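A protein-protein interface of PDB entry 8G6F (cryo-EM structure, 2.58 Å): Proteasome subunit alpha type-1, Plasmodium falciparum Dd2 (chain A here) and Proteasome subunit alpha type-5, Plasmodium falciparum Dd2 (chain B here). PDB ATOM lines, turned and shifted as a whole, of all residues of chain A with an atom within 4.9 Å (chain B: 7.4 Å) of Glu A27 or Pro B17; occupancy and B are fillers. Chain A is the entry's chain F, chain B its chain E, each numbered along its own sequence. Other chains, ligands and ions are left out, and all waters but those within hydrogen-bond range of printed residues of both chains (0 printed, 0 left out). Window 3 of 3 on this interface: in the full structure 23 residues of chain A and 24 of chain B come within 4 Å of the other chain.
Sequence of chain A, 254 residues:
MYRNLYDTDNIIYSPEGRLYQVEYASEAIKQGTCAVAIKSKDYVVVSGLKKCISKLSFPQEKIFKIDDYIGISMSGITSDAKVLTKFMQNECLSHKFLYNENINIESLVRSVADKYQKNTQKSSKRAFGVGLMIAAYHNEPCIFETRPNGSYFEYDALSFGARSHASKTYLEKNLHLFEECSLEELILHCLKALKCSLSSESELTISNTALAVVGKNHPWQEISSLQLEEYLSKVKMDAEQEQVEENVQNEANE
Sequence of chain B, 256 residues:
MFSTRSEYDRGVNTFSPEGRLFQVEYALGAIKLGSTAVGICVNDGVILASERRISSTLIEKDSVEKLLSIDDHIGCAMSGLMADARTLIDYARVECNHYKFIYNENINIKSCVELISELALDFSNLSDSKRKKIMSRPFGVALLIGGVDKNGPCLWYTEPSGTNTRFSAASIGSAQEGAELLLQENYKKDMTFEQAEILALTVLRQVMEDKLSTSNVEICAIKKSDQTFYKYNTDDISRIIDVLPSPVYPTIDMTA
O of Phe B15 touches CD2 of Tyr A24 (3.7 Å).
Tyr A24 touches Ser B16.
Tyr A24 touches Pro B17 (CD2 to CA, 3.8 Å).
Gly B19 touches Tyr A24 (CA to O, 3.3 Å).
CE2 of Phe B15 touches CB of Ala A25, at 3.8 Å.
CG of Glu A27 touches O of Pro B17, at 3.7 Å.
C of Glu B18 touches CG of Glu A27 (3.99 Å).
Gly B19 touches Ala A28.
Of the 8 printed residues of chain B, 5 touch a printed residue of chain A.
Printed residues of chain B that touch a printed residue of chain A: Phe B15, Ser B16, Pro B17, Glu B18 and Gly B19.
Hydrophobic or aromatic side chains of chain B that line the printed part of chain A: Phe B15 and Pro B17.
Hydrophobic or aromatic side chains of chain A within 4 Å of the printed part of chain B: Tyr A24, Ala A25 and Ala A28.
Along chain A the printed residues that touch a printed residue of chain B span positions 24 to 28.
Among the printed residues, 8 pairs touch across the chains.
Among the printed residues, no Asp or Glu carboxylate lies within 4 Å of a Lys or Arg side-chain nitrogen of the other chain.
The backbone carbonyl oxygen (O) of Glu A27 sits at hydrogen-bond distance from the side-chain amide nitrogen (NE2) of Gln A31 (3.3 Å).
The side-chain hydroxyl (OG) of Ser B16 lies close to the backbone NH (N) of Glu B18.
The backbone NH of Arg B20 sits at hydrogen-bond distance from the side-chain hydroxyl of Ser B16, at 3.3 Å.
Printed residues of chain A within 4 Å of Phe B15: Tyr A24 and Ala A25.
Of the printed residues of chain A, Glu B18 touches Glu A27 (3.99 Å).
Printed residues of chain B within 4 Å of Tyr A24: Phe B15 (3.7 Å), Ser B16 (3.4 Å), Pro B17 (3.8 Å) and Gly B19 (3.3 Å).
Of the printed residues of chain B, Ala A25 touches Phe B15.
Of the printed residues of chain B, Ala A28 touches Gly B19.
Arg B10 touches none of the printed residues of chain A.
Ser A26 touches none of the printed residues of chain B.
The nearest printed residue of chain B that does not touch Glu A27 is Gly B19 (4.3 Å).
The nearest printed residue of chain A that does not touch Pro B17 is Glu A23 (6.2 Å).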
ATOM      1  N   GLU A  23     -13.964  -2.877 -21.658  1.00  0.00           N
ATOM      2  CA  GLU A  23     -15.354  -2.556 -21.352  1.00  0.00           C
ATOM      3  C   GLU A  23     -15.457  -1.281 -20.523  1.00  0.00           C
ATOM      4  O   GLU A  23     -16.397  -0.502 -20.685  1.00  0.00           O
ATOM      5  CB  GLU A  23     -16.011  -3.722 -20.620  1.00  0.00           C
ATOM      6  CG  GLU A  23     -16.188  -4.958 -21.474  1.00  0.00           C
ATOM      7  CD  GLU A  23     -17.029  -6.008 -20.791  1.00  0.00           C
ATOM      8  OE1 GLU A  23     -17.297  -5.856 -19.582  1.00  0.00           O
ATOM      9  OE2 GLU A  23     -17.426  -6.984 -21.458  1.00  0.00           O
ATOM     10  N   TYR A  24     -14.501  -1.051 -19.625  1.00  0.00           N
ATOM     11  CA  TYR A  24     -14.522   0.165 -18.815  1.00  0.00           C
ATOM     12  C   TYR A  24     -14.133   1.384 -19.643  1.00  0.00           C
ATOM     13  O   TYR A  24     -14.681   2.479 -19.457  1.00  0.00           O
ATOM     14  CB  TYR A  24     -13.589   0.008 -17.616  1.00  0.00           C
ATOM     15  CG  TYR A  24     -13.957  -1.129 -16.687  1.00  0.00           C
ATOM     16  CD1 TYR A  24     -15.212  -1.717 -16.737  1.00  0.00           C
ATOM     17  CD2 TYR A  24     -13.049  -1.608 -15.756  1.00  0.00           C
ATOM     18  CE1 TYR A  24     -15.550  -2.746 -15.892  1.00  0.00           C
ATOM     19  CE2 TYR A  24     -13.381  -2.639 -14.906  1.00  0.00           C
ATOM     20  CZ  TYR A  24     -14.633  -3.203 -14.981  1.00  0.00           C
ATOM     21  OH  TYR A  24     -14.976  -4.230 -14.137  1.00  0.00           O
ATOM     22  N   ALA A  25     -13.183   1.215 -20.561  1.00  0.00           N
ATOM     23  CA  ALA A  25     -12.917   2.275 -21.525  1.00  0.00           C
ATOM     24  C   ALA A  25     -14.190   2.651 -22.276  1.00  0.00           C
ATOM     25  O   ALA A  25     -14.454   3.833 -22.516  1.00  0.00           O
ATOM     26  CB  ALA A  25     -11.824   1.839 -22.496  1.00  0.00           C
ATOM     27  N   SER A  26     -14.992   1.656 -22.655  1.00  0.00           N
ATOM     28  CA  SER A  26     -16.271   1.948 -23.299  1.00  0.00           C
ATOM     29  C   SER A  26     -17.240   2.617 -22.331  1.00  0.00           C
ATOM     30  O   SER A  26     -18.015   3.493 -22.725  1.00  0.00           O
ATOM     31  CB  SER A  26     -16.879   0.667 -23.863  1.00  0.00           C
ATOM     32  OG  SER A  26     -15.945  -0.027 -24.669  1.00  0.00           O
ATOM     33  N   GLU A  27     -17.224   2.198 -21.067  1.00  0.00           N
ATOM     34  CA  GLU A  27     -18.073   2.823 -20.060  1.00  0.00           C
ATOM     35  C   GLU A  27     -17.787   4.309 -19.943  1.00  0.00           C
ATOM     36  O   GLU A  27     -18.687   5.098 -19.642  1.00  0.00           O
ATOM     37  CB  GLU A  27     -17.862   2.137 -18.712  1.00  0.00           C
ATOM     38  CG  GLU A  27     -18.807   2.579 -17.620  1.00  0.00           C
ATOM     39  CD  GLU A  27     -20.211   2.046 -17.819  1.00  0.00           C
ATOM     40  OE1 GLU A  27     -20.356   0.910 -18.316  1.00  0.00           O
ATOM     41  OE2 GLU A  27     -21.170   2.763 -17.466  1.00  0.00           O
ATOM     42  N   ALA A  28     -16.535   4.705 -20.162  1.00  0.00           N
ATOM     43  CA  ALA A  28     -16.201   6.125 -20.129  1.00  0.00           C
ATOM     44  C   ALA A  28     -17.006   6.916 -21.154  1.00  0.00           C
ATOM     45  O   ALA A  28     -17.254   8.109 -20.958  1.00  0.00           O
ATOM     46  CB  ALA A  28     -14.708   6.319 -20.377  1.00  0.00           C
ATOM     47  N   ILE A  29     -17.418   6.273 -22.246  1.00  0.00           N
ATOM     48  CA  ILE A  29     -18.124   6.974 -23.315  1.00  0.00           C
ATOM     49  C   ILE A  29     -19.522   7.374 -22.871  1.00  0.00           C
ATOM     50  O   ILE A  29     -20.010   8.456 -23.214  1.00  0.00           O
ATOM     51  CB  ILE A  29     -18.172   6.095 -24.576  1.00  0.00           C
ATOM     52  CG1 ILE A  29     -16.776   5.963 -25.175  1.00  0.00           C
ATOM     53  CG2 ILE A  29     -19.146   6.673 -25.583  1.00  0.00           C
ATOM     54  CD1 ILE A  29     -16.640   4.820 -26.136  1.00  0.00           C
ATOM     55  N   LYS A  30     -20.197   6.507 -22.120  1.00  0.00           N
ATOM     56  CA  LYS A  30     -21.571   6.766 -21.714  1.00  0.00           C
ATOM     57  C   LYS A  30     -21.699   7.960 -20.781  1.00  0.00           C
ATOM     58  O   LYS A  30     -22.820   8.429 -20.561  1.00  0.00           O
ATOM     59  CB  LYS A  30     -22.153   5.529 -21.034  1.00  0.00           C
ATOM     60  CG  LYS A  30     -22.131   4.282 -21.894  1.00  0.00           C
ATOM     61  CD  LYS A  30     -22.498   3.054 -21.086  1.00  0.00           C
ATOM     62  CE  LYS A  30     -22.324   1.784 -21.893  1.00  0.00           C
ATOM     63  NZ  LYS A  30     -20.924   1.611 -22.359  1.00  0.00           N
ATOM     64  N   GLN A  31     -20.598   8.453 -20.223  1.00  0.00           N
ATOM     65  CA  GLN A  31     -20.643   9.578 -19.301  1.00  0.00           C
ATOM     66  C   GLN A  31     -20.568  10.931 -19.996  1.00  0.00           C
ATOM     67  O   GLN A  31     -20.761  11.955 -19.333  1.00  0.00           O
ATOM     68  CB  GLN A  31     -19.498   9.476 -18.288  1.00  0.00           C
ATOM     69  CG  GLN A  31     -19.273   8.081 -17.728  1.00  0.00           C
ATOM     70  CD  GLN A  31     -20.522   7.493 -17.112  1.00  0.00           C
ATOM     71  OE1 GLN A  31     -21.309   8.200 -16.488  1.00  0.00           O
ATOM     72  NE2 GLN A  31     -20.711   6.191 -17.283  1.00  0.00           N
ATOM     73  N   ARG B  10      -2.597  -1.688  -8.705  1.00  0.00           N
ATOM     74  CA  ARG B  10      -3.018  -1.322 -10.045  1.00  0.00           C
ATOM     75  C   ARG B  10      -1.902  -0.593 -10.777  1.00  0.00           C
ATOM     76  O   ARG B  10      -1.062   0.074 -10.167  1.00  0.00           O
ATOM     77  CB  ARG B  10      -4.261  -0.434  -9.995  1.00  0.00           C
ATOM     78  CG  ARG B  10      -5.241  -0.787  -8.899  1.00  0.00           C
ATOM     79  CD  ARG B  10      -6.659  -0.503  -9.341  1.00  0.00           C
ATOM     80  NE  ARG B  10      -7.612  -0.536  -8.241  1.00  0.00           N
ATOM     81  CZ  ARG B  10      -7.681   0.376  -7.281  1.00  0.00           C
ATOM     82  NH1 ARG B  10      -6.847   1.402  -7.240  1.00  0.00           N
ATOM     83  NH2 ARG B  10      -8.611   0.256  -6.338  1.00  0.00           N
ATOM     84  N   PHE B  15      -8.226   1.362 -15.711  1.00  0.00           N
ATOM     85  CA  PHE B  15      -9.537   1.992 -15.720  1.00  0.00           C
ATOM     86  C   PHE B  15     -10.350   1.491 -14.537  1.00  0.00           C
ATOM     87  O   PHE B  15     -10.290   0.311 -14.187  1.00  0.00           O
ATOM     88  CB  PHE B  15     -10.285   1.672 -17.016  1.00  0.00           C
ATOM     89  CG  PHE B  15     -10.071   2.669 -18.108  1.00  0.00           C
ATOM     90  CD1 PHE B  15     -10.615   3.934 -18.027  1.00  0.00           C
ATOM     91  CD2 PHE B  15      -9.336   2.335 -19.227  1.00  0.00           C
ATOM     92  CE1 PHE B  15     -10.422   4.849 -19.038  1.00  0.00           C
ATOM     93  CE2 PHE B  15      -9.139   3.246 -20.238  1.00  0.00           C
ATOM     94  CZ  PHE B  15      -9.683   4.504 -20.144  1.00  0.00           C
ATOM     95  N   SER B  16     -11.105   2.387 -13.923  1.00  0.00           N
ATOM     96  CA  SER B  16     -12.052   1.979 -12.903  1.00  0.00           C
ATOM     97  C   SER B  16     -13.346   1.502 -13.555  1.00  0.00           C
ATOM     98  O   SER B  16     -13.635   1.846 -14.702  1.00  0.00           O
ATOM     99  CB  SER B  16     -12.335   3.133 -11.950  1.00  0.00           C
ATOM    100  OG  SER B  16     -13.308   4.005 -12.485  1.00  0.00           O
ATOM    101  N   PRO B  17     -14.147   0.707 -12.845  1.00  0.00           N
ATOM    102  CA  PRO B  17     -15.394   0.208 -13.447  1.00  0.00           C
ATOM    103  C   PRO B  17     -16.324   1.307 -13.918  1.00  0.00           C
ATOM    104  O   PRO B  17     -17.239   1.027 -14.700  1.00  0.00           O
ATOM    105  CB  PRO B  17     -16.026  -0.614 -12.317  1.00  0.00           C
ATOM    106  CG  PRO B  17     -14.896  -0.985 -11.439  1.00  0.00           C
ATOM    107  CD  PRO B  17     -13.929   0.151 -11.501  1.00  0.00           C
ATOM    108  N   GLU B  18     -16.127   2.542 -13.463  1.00  0.00           N
ATOM    109  CA  GLU B  18     -16.919   3.682 -13.900  1.00  0.00           C
ATOM    110  C   GLU B  18     -16.313   4.401 -15.098  1.00  0.00           C
ATOM    111  O   GLU B  18     -16.860   5.419 -15.531  1.00  0.00           O
ATOM    112  CB  GLU B  18     -17.088   4.672 -12.745  1.00  0.00           C
ATOM    113  CG  GLU B  18     -18.039   4.200 -11.663  1.00  0.00           C
ATOM    114  CD  GLU B  18     -17.403   3.201 -10.718  1.00  0.00           C
ATOM    115  OE1 GLU B  18     -16.176   3.279 -10.502  1.00  0.00           O
ATOM    116  OE2 GLU B  18     -18.131   2.336 -10.189  1.00  0.00           O
ATOM    117  N   GLY B  19     -15.204   3.908 -15.639  1.00  0.00           N
ATOM    118  CA  GLY B  19     -14.607   4.504 -16.815  1.00  0.00           C
ATOM    119  C   GLY B  19     -13.604   5.598 -16.549  1.00  0.00           C
ATOM    120  O   GLY B  19     -13.324   6.390 -17.453  1.00  0.00           O
ATOM    121  N   ARG B  20     -13.053   5.673 -15.341  1.00  0.00           N
ATOM    122  CA  ARG B  20     -12.116   6.717 -14.964  1.00  0.00           C
ATOM    123  C   ARG B  20     -10.761   6.111 -14.632  1.00  0.00           C
ATOM    124  O   ARG B  20     -10.660   4.936 -14.275  1.00  0.00           O
ATOM    125  CB  ARG B  20     -12.630   7.508 -13.763  1.00  0.00           C
ATOM    126  CG  ARG B  20     -13.999   8.116 -13.967  1.00  0.00           C
ATOM    127  CD  ARG B  20     -14.270   9.206 -12.950  1.00  0.00           C
ATOM    128  NE  ARG B  20     -15.523   9.902 -13.218  1.00  0.00           N
ATOM    129  CZ  ARG B  20     -16.727   9.387 -13.014  1.00  0.00           C
ATOM    130  NH1 ARG B  20     -16.886   8.159 -12.548  1.00  0.00           N
ATOM    131  NH2 ARG B  20     -17.801  10.123 -13.286  1.00  0.00           N
ATOM    132  N   PHE B  22      -7.654   5.799 -12.219  1.00  0.00           N
ATOM    133  CA  PHE B  22      -7.435   5.955 -10.785  1.00  0.00           C
ATOM    134  C   PHE B  22      -6.388   7.020 -10.498  1.00  0.00           C
ATOM    135  O   PHE B  22      -6.548   7.826  -9.575  1.00  0.00           O
ATOM    136  CB  PHE B  22      -6.999   4.622 -10.179  1.00  0.00           C
ATOM    137  CG  PHE B  22      -8.084   3.593 -10.122  1.00  0.00           C
ATOM    138  CD1 PHE B  22      -9.152   3.739  -9.260  1.00  0.00           C
ATOM    139  CD2 PHE B  22      -8.028   2.468 -10.922  1.00  0.00           C
ATOM    140  CE1 PHE B  22     -10.144   2.788  -9.202  1.00  0.00           C
ATOM    141  CE2 PHE B  22      -9.018   1.515 -10.866  1.00  0.00           C
ATOM    142  CZ  PHE B  22     -10.076   1.675 -10.006  1.00  0.00           C
